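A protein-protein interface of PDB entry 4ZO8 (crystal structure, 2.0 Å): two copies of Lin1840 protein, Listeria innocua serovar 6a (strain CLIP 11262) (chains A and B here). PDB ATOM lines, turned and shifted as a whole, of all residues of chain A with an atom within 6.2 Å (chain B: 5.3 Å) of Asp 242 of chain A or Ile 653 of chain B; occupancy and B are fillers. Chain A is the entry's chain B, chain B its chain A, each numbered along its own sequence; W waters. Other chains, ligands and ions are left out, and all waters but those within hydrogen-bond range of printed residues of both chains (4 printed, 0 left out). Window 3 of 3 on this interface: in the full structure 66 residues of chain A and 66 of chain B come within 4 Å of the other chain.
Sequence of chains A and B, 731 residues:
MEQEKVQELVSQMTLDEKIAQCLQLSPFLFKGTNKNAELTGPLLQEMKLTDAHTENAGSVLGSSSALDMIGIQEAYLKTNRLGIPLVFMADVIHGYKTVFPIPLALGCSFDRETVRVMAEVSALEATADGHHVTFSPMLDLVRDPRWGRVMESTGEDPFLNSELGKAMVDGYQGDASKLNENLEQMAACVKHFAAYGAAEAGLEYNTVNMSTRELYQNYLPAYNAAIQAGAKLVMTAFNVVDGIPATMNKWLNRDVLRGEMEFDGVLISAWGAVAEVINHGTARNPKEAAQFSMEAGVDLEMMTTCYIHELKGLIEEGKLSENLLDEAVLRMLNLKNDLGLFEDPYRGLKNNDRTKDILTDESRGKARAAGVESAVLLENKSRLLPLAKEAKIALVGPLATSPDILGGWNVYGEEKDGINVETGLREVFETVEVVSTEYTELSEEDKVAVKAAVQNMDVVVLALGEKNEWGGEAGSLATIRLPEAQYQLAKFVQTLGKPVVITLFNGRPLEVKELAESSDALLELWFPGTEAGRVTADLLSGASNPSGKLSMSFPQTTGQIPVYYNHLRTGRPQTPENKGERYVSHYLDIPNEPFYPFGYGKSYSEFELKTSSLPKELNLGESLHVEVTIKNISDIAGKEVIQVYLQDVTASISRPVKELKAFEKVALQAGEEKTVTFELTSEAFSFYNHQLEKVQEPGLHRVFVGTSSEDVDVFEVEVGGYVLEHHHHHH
Of the 13 printed residues of chain A, 8 touch a printed residue of chain B.
Printed residues of chain A that touch a printed residue of chain B: Asn 209, Met 210, Asp 242, Gly 243, Ile 244, His 280, Gly 281 and Thr 282.
Hydrophobic or aromatic side chains of chain A within 4 Å of the printed part of chain B: Ile 244.
Printed residues of chain B that touch a printed residue of chain A: Ser 211, Arg 213, Glu 214, Ala 651, Ser 652, Ile 653 and Ser 654.
Among the printed residues, 17 pairs touch across the chains.
The side-chain hydroxyl of Ser 211 of chain B lies close to the backbone NH of Arg 213 of chain B, at 3.4 Å.
The backbone NH of Glu 214 of chain B lies within hydrogen-bond range of the side-chain hydroxyl of Ser 211 of chain B (3.0 Å).
The guanidinium group (NH1) of Arg 213 of chain B lies within salt-bridge range of the side-chain carboxylate (OE1) of Glu 214 of chain B.
The backbone carbonyl oxygen of Ile 244 of chain A lies close to the side-chain amide nitrogen of Asn 249 of chain A.
Among the printed residues, pairs that only touch across the chains: Asn 209 of chain A with Arg 213 of chain B (3.8 Å), Asn 209 of chain A with Glu 214 of chain B (3.4 Å), Met 210 of chain A with Ser 211 of chain B (3.7 Å), Asp 242 of chain A with Ile 653 of chain B (3.9 Å), Gly 243 of chain A with Arg 213 of chain B (3.6 Å), Gly 243 of chain A with Ile 653 of chain B (3.6 Å), Ile 244 of chain A with Ser 652 of chain B (2.8 Å), Ile 244 of chain A with Ile 653 of chain B (3.3 Å), Thr 282 of chain A with Ala 651 of chain B (3.2 Å), Thr 282 of chain A with Ile 653 of chain B (3.8 Å) and Thr 282 of chain A with Ser 654 of chain B (3.6 Å).
Asp 242 of chain A touches just these residues of chain B: Ser 211, Arg 213 and Ile 653.
Of the printed residues of chain A, Ile 653 of chain B touches Asp 242 (3.9 Å), Gly 243 (3.6 Å), Ile 244 (3.3 Å) and Thr 282 (3.8 Å).
Of the printed residues of chain B, Met 210 of chain A touches Ser 211 (3.7 Å).
Of the printed residues of chain A, Ala 651 of chain B touches Gly 281 and Thr 282.
Of the printed residues of chain A, Ser 652 of chain B touches Ile 244.
Of the printed residues of chain A, Arg 213 of chain B touches Asn 209, Asp 242 and Gly 243.
Of the printed residues of chain B, Asn 209 of chain A touches Ser 211, Arg 213 and Glu 214.
Val 208 of chain A touches none of the printed residues of chain B.
Asn 689 of chain B touches none of the printed residues of chain A.
The nearest residue of chain B that does not touch Asp 242 of chain A is Glu 214 of chain B (4.8 Å).
The nearest residue of chain A that does not touch Ile 653 of chain B is Gly 281 of chain A (4.5 Å).
The backbone NH (N) of Ser 211 of chain B lies within hydrogen-bond range of the side-chain amide oxygen (OD1) of Asn 209 of chain A, 2.9 Å away.
The side-chain hydroxyl (OG) of Ser 211 of chain B is in hydrogen-bond range of the side-chain carboxylate (OD1) of Asp 242 of chain A, 2.6 Å away.
The guanidinium group (NH2) of Arg 213 of chain B lies within salt-bridge range of the side-chain carboxylate (OD1) of Asp 242 of chain A (3.0 Å).
N of Ala 651 of chain B sits at hydrogen-bond distance from O of Gly 281 of chain A, at 2.7 Å.
The backbone NH (N) of Ser 654 of chain B lies within hydrogen-bond range of the backbone carbonyl oxygen (O) of Gly 243 of chain A, 2.8 Å away.
OG of Ser 654 of chain B is in hydrogen-bond range of O of His 280 of chain A, at 2.7 Å.
Water W3 lies within hydrogen-bond range of OD2 of Asp 242 of chain A, N of Arg 213 of chain B and N of Thr 212 of chain B.
Water W2 bridges the side-chain hydroxyl of Ser 654 of chain B and a ring nitrogen (ND1) of His 280 of chain A.
Water W1 bridges O of Gly 281 of chain A and N of Arg 655 of chain B.
Water W4 lies within hydrogen-bond range of the backbone NH of Thr 212 of chain B (3.1 Å) and the backbone NH of Thr 212 of chain A (3.2 Å).
Position printed for both chains: 212.
Of the 17 pairs that touch across the chains among the printed residues, none has its exchanged pair printed and touching as well.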
ATOM      1  N   VAL A 208     -12.577 -20.813  -4.747  1.00  0.00           N
ATOM      2  CA  VAL A 208     -12.381 -22.250  -4.647  1.00  0.00           C
ATOM      3  C   VAL A 208     -13.235 -22.725  -3.485  1.00  0.00           C
ATOM      4  O   VAL A 208     -13.246 -22.112  -2.423  1.00  0.00           O
ATOM      5  CB  VAL A 208     -10.882 -22.574  -4.424  1.00  0.00           C
ATOM      6  CG1 VAL A 208     -10.684 -24.038  -3.971  1.00  0.00           C
ATOM      7  CG2 VAL A 208     -10.063 -22.242  -5.687  1.00  0.00           C
ATOM      8  N   ASN A 209     -13.964 -23.811  -3.678  1.00  0.00           N
ATOM      9  CA  ASN A 209     -14.694 -24.446  -2.570  1.00  0.00           C
ATOM     10  C   ASN A 209     -14.842 -25.936  -2.781  1.00  0.00           C
ATOM     11  O   ASN A 209     -15.158 -26.333  -3.854  1.00  0.00           O
ATOM     12  CB  ASN A 209     -16.102 -23.849  -2.415  1.00  0.00           C
ATOM     13  CG  ASN A 209     -16.767 -24.265  -1.114  1.00  0.00           C
ATOM     14  OD1 ASN A 209     -17.615 -25.117  -1.108  1.00  0.00           O
ATOM     15  ND2 ASN A 209     -16.358 -23.662  -0.001  1.00  0.00           N
ATOM     16  N   MET A 210     -14.587 -26.693  -1.730  1.00  0.00           N
ATOM     17  CA  MET A 210     -14.723 -28.140  -1.702  1.00  0.00           C
ATOM     18  C   MET A 210     -14.747 -28.568  -0.231  1.00  0.00           C
ATOM     19  O   MET A 210     -14.292 -27.851   0.610  1.00  0.00           O
ATOM     20  CB  MET A 210     -13.556 -28.818  -2.417  1.00  0.00           C
ATOM     21  CG  MET A 210     -12.350 -28.844  -1.538  1.00  0.00           C
ATOM     22  SD  MET A 210     -10.814 -28.649  -2.400  1.00  0.00           S
ATOM     23  CE  MET A 210     -10.961 -26.889  -2.629  1.00  0.00           C
ATOM     24  N   THR A 212     -13.565 -30.334   3.229  1.00  0.00           N
ATOM     25  CA  THR A 212     -12.240 -30.598   3.815  1.00  0.00           C
ATOM     26  C   THR A 212     -11.763 -32.010   3.437  1.00  0.00           C
ATOM     27  O   THR A 212     -10.634 -32.210   3.040  1.00  0.00           O
ATOM     28  CB  THR A 212     -12.297 -30.436   5.325  1.00  0.00           C
ATOM     29  OG1 THR A 212     -13.039 -29.251   5.620  1.00  0.00           O
ATOM     30  CG2 THR A 212     -10.891 -30.365   5.887  1.00  0.00           C
ATOM     31  N   VAL A 240      -9.322 -18.252  -1.915  1.00  0.00           N
ATOM     32  CA  VAL A 240      -9.855 -18.701  -0.647  1.00  0.00           C
ATOM     33  C   VAL A 240      -9.794 -20.187  -0.529  1.00  0.00           C
ATOM     34  O   VAL A 240      -9.865 -20.876  -1.495  1.00  0.00           O
ATOM     35  CB  VAL A 240     -11.294 -18.266  -0.433  1.00  0.00           C
ATOM     36  CG1 VAL A 240     -11.380 -16.746  -0.367  1.00  0.00           C
ATOM     37  CG2 VAL A 240     -12.252 -18.805  -1.511  1.00  0.00           C
ATOM     38  N   VAL A 241      -9.598 -20.673   0.689  1.00  0.00           N
ATOM     39  CA  VAL A 241      -9.790 -22.056   1.016  1.00  0.00           C
ATOM     40  C   VAL A 241     -10.857 -22.088   2.102  1.00  0.00           C
ATOM     41  O   VAL A 241     -10.700 -21.531   3.170  1.00  0.00           O
ATOM     42  CB  VAL A 241      -8.490 -22.673   1.530  1.00  0.00           C
ATOM     43  CG1 VAL A 241      -8.742 -23.985   2.251  1.00  0.00           C
ATOM     44  CG2 VAL A 241      -7.503 -22.844   0.378  1.00  0.00           C
ATOM     45  N   ASP A 242     -11.944 -22.769   1.832  1.00  0.00           N
ATOM     46  CA  ASP A 242     -13.141 -22.648   2.595  1.00  0.00           C
ATOM     47  C   ASP A 242     -13.392 -21.269   3.167  1.00  0.00           C
ATOM     48  O   ASP A 242     -13.649 -21.109   4.355  1.00  0.00           O
ATOM     49  CB  ASP A 242     -13.209 -23.714   3.696  1.00  0.00           C
ATOM     50  CG  ASP A 242     -14.625 -24.034   4.111  1.00  0.00           C
ATOM     51  OD1 ASP A 242     -15.593 -23.542   3.473  1.00  0.00           O
ATOM     52  OD2 ASP A 242     -14.782 -24.775   5.100  1.00  0.00           O
ATOM     53  N   GLY A 243     -13.398 -20.275   2.292  1.00  0.00           N
ATOM     54  CA  GLY A 243     -13.829 -18.966   2.648  1.00  0.00           C
ATOM     55  C   GLY A 243     -12.743 -18.061   3.172  1.00  0.00           C
ATOM     56  O   GLY A 243     -13.010 -16.884   3.366  1.00  0.00           O
ATOM     57  N   ILE A 244     -11.546 -18.592   3.426  1.00  0.00           N
ATOM     58  CA  ILE A 244     -10.448 -17.773   3.980  1.00  0.00           C
ATOM     59  C   ILE A 244      -9.328 -17.785   3.005  1.00  0.00           C
ATOM     60  O   ILE A 244      -8.824 -18.864   2.699  1.00  0.00           O
ATOM     61  CB  ILE A 244      -9.864 -18.320   5.332  1.00  0.00           C
ATOM     62  CG1 ILE A 244     -10.954 -18.773   6.305  1.00  0.00           C
ATOM     63  CG2 ILE A 244      -8.919 -17.331   5.991  1.00  0.00           C
ATOM     64  CD1 ILE A 244     -11.954 -17.745   6.566  1.00  0.00           C
ATOM     65  N   ASN A 249      -4.813 -17.974   6.241  1.00  0.00           N
ATOM     66  CA  ASN A 249      -5.598 -19.098   6.712  1.00  0.00           C
ATOM     67  C   ASN A 249      -4.772 -19.862   7.732  1.00  0.00           C
ATOM     68  O   ASN A 249      -3.842 -20.650   7.382  1.00  0.00           O
ATOM     69  CB  ASN A 249      -6.066 -19.957   5.547  1.00  0.00           C
ATOM     70  CG  ASN A 249      -7.069 -20.991   5.967  1.00  0.00           C
ATOM     71  OD1 ASN A 249      -6.929 -21.582   7.001  1.00  0.00           O
ATOM     72  ND2 ASN A 249      -8.100 -21.227   5.136  1.00  0.00           N
ATOM     73  N   HIS A 280     -10.121  -9.372  -0.731  1.00  0.00           N
ATOM     74  CA  HIS A 280     -10.954 -10.541  -0.477  1.00  0.00           C
ATOM     75  C   HIS A 280     -11.969 -10.238   0.619  1.00  0.00           C
ATOM     76  O   HIS A 280     -12.904 -11.011   0.836  1.00  0.00           O
ATOM     77  CB  HIS A 280     -10.131 -11.690   0.042  1.00  0.00           C
ATOM     78  CG  HIS A 280      -9.546 -12.611  -0.990  1.00  0.00           C
ATOM     79  ND1 HIS A 280     -10.293 -13.540  -1.687  1.00  0.00           N
ATOM     80  CD2 HIS A 280      -8.261 -12.861  -1.294  1.00  0.00           C
ATOM     81  CE1 HIS A 280      -9.488 -14.300  -2.395  1.00  0.00           C
ATOM     82  NE2 HIS A 280      -8.247 -13.907  -2.181  1.00  0.00           N
ATOM     83  N   GLY A 281     -11.760  -9.151   1.356  1.00  0.00           N
ATOM     84  CA  GLY A 281     -12.697  -8.777   2.436  1.00  0.00           C
ATOM     85  C   GLY A 281     -12.513  -9.528   3.748  1.00  0.00           C
ATOM     86  O   GLY A 281     -13.425  -9.663   4.513  1.00  0.00           O
ATOM     87  N   THR A 282     -11.307 -10.004   4.028  1.00  0.00           N
ATOM     88  CA  THR A 282     -11.020 -10.646   5.288  1.00  0.00           C
ATOM     89  C   THR A 282      -9.970  -9.916   6.126  1.00  0.00           C
ATOM     90  O   THR A 282      -9.469 -10.432   7.132  1.00  0.00           O
ATOM     91  CB  THR A 282     -10.626 -12.156   5.086  1.00  0.00           C
ATOM     92  OG1 THR A 282      -9.503 -12.251   4.233  1.00  0.00           O
ATOM     93  CG2 THR A 282     -11.760 -12.952   4.482  1.00  0.00           C
ATOM     94  N   SER B 211     -18.017 -27.268   0.825  1.00  0.00           N
ATOM     95  CA  SER B 211     -17.685 -27.294   2.240  1.00  0.00           C
ATOM     96  C   SER B 211     -18.971 -27.342   3.046  1.00  0.00           C
ATOM     97  O   SER B 211     -20.049 -26.842   2.636  1.00  0.00           O
ATOM     98  CB  SER B 211     -16.844 -26.083   2.639  1.00  0.00           C
ATOM     99  OG  SER B 211     -17.637 -24.881   2.700  1.00  0.00           O
ATOM    100  N   THR B 212     -18.864 -27.919   4.237  1.00  0.00           N
ATOM    101  CA  THR B 212     -19.989 -27.900   5.153  1.00  0.00           C
ATOM    102  C   THR B 212     -20.468 -26.453   5.385  1.00  0.00           C
ATOM    103  O   THR B 212     -21.673 -26.182   5.413  1.00  0.00           O
ATOM    104  CB  THR B 212     -19.604 -28.601   6.462  1.00  0.00           C
ATOM    105  OG1 THR B 212     -18.890 -29.817   6.159  1.00  0.00           O
ATOM    106  CG2 THR B 212     -20.858 -28.922   7.257  1.00  0.00           C
ATOM    107  N   ARG B 213     -19.554 -25.501   5.495  1.00  0.00           N
ATOM    108  CA  ARG B 213     -19.959 -24.096   5.714  1.00  0.00           C
ATOM    109  C   ARG B 213     -20.809 -23.499   4.591  1.00  0.00           C
ATOM    110  O   ARG B 213     -21.851 -22.838   4.835  1.00  0.00           O
ATOM    111  CB  ARG B 213     -18.705 -23.215   5.904  1.00  0.00           C
ATOM    112  CG  ARG B 213     -19.042 -21.775   6.226  1.00  0.00           C
ATOM    113  CD  ARG B 213     -17.810 -20.897   6.230  1.00  0.00           C
ATOM    114  NE  ARG B 213     -17.111 -21.057   4.982  1.00  0.00           N
ATOM    115  CZ  ARG B 213     -17.611 -20.720   3.792  1.00  0.00           C
ATOM    116  NH1 ARG B 213     -18.812 -20.099   3.704  1.00  0.00           N
ATOM    117  NH2 ARG B 213     -16.895 -20.966   2.681  1.00  0.00           N
ATOM    118  N   GLU B 214     -20.403 -23.786   3.351  1.00  0.00           N
ATOM    119  CA  GLU B 214     -21.225 -23.432   2.172  1.00  0.00           C
ATOM    120  C   GLU B 214     -22.573 -24.147   2.134  1.00  0.00           C
ATOM    121  O   GLU B 214     -23.610 -23.586   1.775  1.00  0.00           O
ATOM    122  CB  GLU B 214     -20.468 -23.770   0.895  1.00  0.00           C
ATOM    123  CG  GLU B 214     -19.581 -22.614   0.474  1.00  0.00           C
ATOM    124  CD  GLU B 214     -20.423 -21.371   0.176  1.00  0.00           C
ATOM    125  OE1 GLU B 214     -20.274 -20.368   0.941  1.00  0.00           O
ATOM    126  OE2 GLU B 214     -21.288 -21.453  -0.774  1.00  0.00           O
ATOM    127  N   ALA B 651     -14.943  -9.466   6.759  1.00  0.00           N
ATOM    128  CA  ALA B 651     -15.445 -10.471   7.667  1.00  0.00           C
ATOM    129  C   ALA B 651     -14.425 -11.590   7.816  1.00  0.00           C
ATOM    130  O   ALA B 651     -13.435 -11.584   7.149  1.00  0.00           O
ATOM    131  CB  ALA B 651     -16.805 -10.991   7.175  1.00  0.00           C
ATOM    132  N   SER B 652     -14.639 -12.467   8.785  1.00  0.00           N
ATOM    133  CA  SER B 652     -13.741 -13.605   9.022  1.00  0.00           C
ATOM    134  C   SER B 652     -13.862 -14.715   7.962  1.00  0.00           C
ATOM    135  O   SER B 652     -13.024 -15.589   7.917  1.00  0.00           O
ATOM    136  CB  SER B 652     -13.975 -14.196  10.406  1.00  0.00           C
ATOM    137  OG  SER B 652     -15.300 -14.681  10.492  1.00  0.00           O
ATOM    138  N   ILE B 653     -14.913 -14.661   7.151  1.00  0.00           N
ATOM    139  CA  ILE B 653     -15.075 -15.442   5.910  1.00  0.00           C
ATOM    140  C   ILE B 653     -15.301 -14.390   4.790  1.00  0.00           C
ATOM    141  O   ILE B 653     -15.905 -13.332   5.042  1.00  0.00           O
ATOM    142  CB  ILE B 653     -16.321 -16.329   6.014  1.00  0.00           C
ATOM    143  CG1 ILE B 653     -16.170 -17.342   7.143  1.00  0.00           C
ATOM    144  CG2 ILE B 653     -16.631 -16.981   4.676  1.00  0.00           C
ATOM    145  CD1 ILE B 653     -15.125 -18.430   6.848  1.00  0.00           C
ATOM    146  N   SER B 654     -14.760 -14.649   3.594  1.00  0.00           N
ATOM    147  CA  SER B 654     -14.887 -13.726   2.488  1.00  0.00           C
ATOM    148  C   SER B 654     -16.357 -13.813   2.095  1.00  0.00           C
ATOM    149  O   SER B 654     -16.830 -14.878   1.794  1.00  0.00           O
ATOM    150  CB  SER B 654     -13.953 -14.128   1.335  1.00  0.00           C
ATOM    151  OG  SER B 654     -14.173 -13.294   0.218  1.00  0.00           O
ATOM    152  N   ARG B 655     -17.086 -12.693   2.210  1.00  0.00           N
ATOM    153  CA  ARG B 655     -18.550 -12.671   2.059  1.00  0.00           C
ATOM    154  C   ARG B 655     -18.952 -12.178   0.663  1.00  0.00           C
ATOM    155  O   ARG B 655     -18.215 -11.481  -0.015  1.00  0.00           O
ATOM    156  CB  ARG B 655     -19.254 -11.816   3.169  1.00  0.00           C
ATOM    157  CG  ARG B 655     -19.019 -12.290   4.612  1.00  0.00           C
ATOM    158  CD  ARG B 655     -20.064 -13.284   5.124  1.00  0.00           C
ATOM    159  NE  ARG B 655     -21.350 -12.652   5.148  1.00  0.00           N
ATOM    160  CZ  ARG B 655     -22.442 -13.102   4.530  1.00  0.00           C
ATOM    161  NH1 ARG B 655     -22.446 -14.220   3.840  1.00  0.00           N
ATOM    162  NH2 ARG B 655     -23.531 -12.398   4.585  1.00  0.00           N
ATOM    163  N   PHE B 687     -23.926 -14.727   9.366  1.00  0.00           N
ATOM    164  CA  PHE B 687     -23.407 -15.740   8.472  1.00  0.00           C
ATOM    165  C   PHE B 687     -22.756 -16.807   9.283  1.00  0.00           C
ATOM    166  O   PHE B 687     -22.449 -16.584  10.448  1.00  0.00           O
ATOM    167  CB  PHE B 687     -22.350 -15.149   7.506  1.00  0.00           C
ATOM    168  CG  PHE B 687     -21.080 -14.724   8.171  1.00  0.00           C
ATOM    169  CD1 PHE B 687     -21.019 -13.523   8.840  1.00  0.00           C
ATOM    170  CD2 PHE B 687     -19.959 -15.479   8.079  1.00  0.00           C
ATOM    171  CE1 PHE B 687     -19.851 -13.136   9.496  1.00  0.00           C
ATOM    172  CE2 PHE B 687     -18.765 -15.074   8.686  1.00  0.00           C
ATOM    173  CZ  PHE B 687     -18.728 -13.916   9.411  1.00  0.00           C
ATOM    174  N   TYR B 688     -22.497 -17.940   8.608  1.00  0.00           N
ATOM    175  CA  TYR B 688     -21.706 -19.025   9.162  1.00  0.00           C
ATOM    176  C   TYR B 688     -20.205 -18.828   9.113  1.00  0.00           C
ATOM    177  O   TYR B 688     -19.625 -18.558   8.050  1.00  0.00           O
ATOM    178  CB  TYR B 688     -22.027 -20.317   8.489  1.00  0.00           C
ATOM    179  CG  TYR B 688     -23.387 -20.744   8.834  1.00  0.00           C
ATOM    180  CD1 TYR B 688     -23.651 -21.487   9.957  1.00  0.00           C
ATOM    181  CD2 TYR B 688     -24.444 -20.340   8.051  1.00  0.00           C
ATOM    182  CE1 TYR B 688     -24.977 -21.872  10.261  1.00  0.00           C
ATOM    183  CE2 TYR B 688     -25.709 -20.679   8.349  1.00  0.00           C
ATOM    184  CZ  TYR B 688     -25.980 -21.456   9.451  1.00  0.00           C
ATOM    185  OH  TYR B 688     -27.303 -21.750   9.635  1.00  0.00           O
ATOM    186  N   ASN B 689     -19.554 -19.061  10.241  1.00  0.00           N
ATOM    187  CA  ASN B 689     -18.108 -18.867  10.297  1.00  0.00           C
ATOM    188  C   ASN B 689     -17.316 -20.143  10.068  1.00  0.00           C
ATOM    189  O   ASN B 689     -17.910 -21.201   9.849  1.00  0.00           O
ATOM    190  CB  ASN B 689     -17.700 -18.126  11.576  1.00  0.00           C
ATOM    191  CG  ASN B 689     -17.844 -18.957  12.842  1.00  0.00           C
ATOM    192  OD1 ASN B 689     -18.036 -20.132  12.802  1.00  0.00           O
ATOM    193  ND2 ASN B 689     -17.706 -18.301  13.987  1.00  0.00           N
ATOM    194  N   HIS B 690     -15.979 -20.061  10.070  1.00  0.00           N
ATOM    195  CA  HIS B 690     -15.137 -21.286   9.754  1.00  0.00           C
ATOM    196  C   HIS B 690     -15.409 -22.396  10.766  1.00  0.00           C
ATOM    197  O   HIS B 690     -15.169 -23.555  10.477  1.00  0.00           O
ATOM    198  CB  HIS B 690     -13.634 -21.025   9.687  1.00  0.00           C
ATOM    199  CG  HIS B 690     -12.984 -20.988  11.021  1.00  0.00           C
ATOM    200  ND1 HIS B 690     -13.131 -19.914  11.880  1.00  0.00           N
ATOM    201  CD2 HIS B 690     -12.235 -21.903  11.677  1.00  0.00           C
ATOM    202  CE1 HIS B 690     -12.488 -20.170  13.007  1.00  0.00           C
ATOM    203  NE2 HIS B 690     -11.932 -21.367  12.907  1.00  0.00           N
HETATM  204  O   HOH W   1     -16.128 -10.071   3.330  1.00  0.00           O
HETATM  205  O   HOH W   2     -13.004 -13.749  -2.241  1.00  0.00           O
HETATM  206  O   HOH W   3     -16.581 -26.095   6.122  1.00  0.00           O
HETATM  207  O   HOH W   4     -16.159 -29.283   4.695  1.00  0.00           O
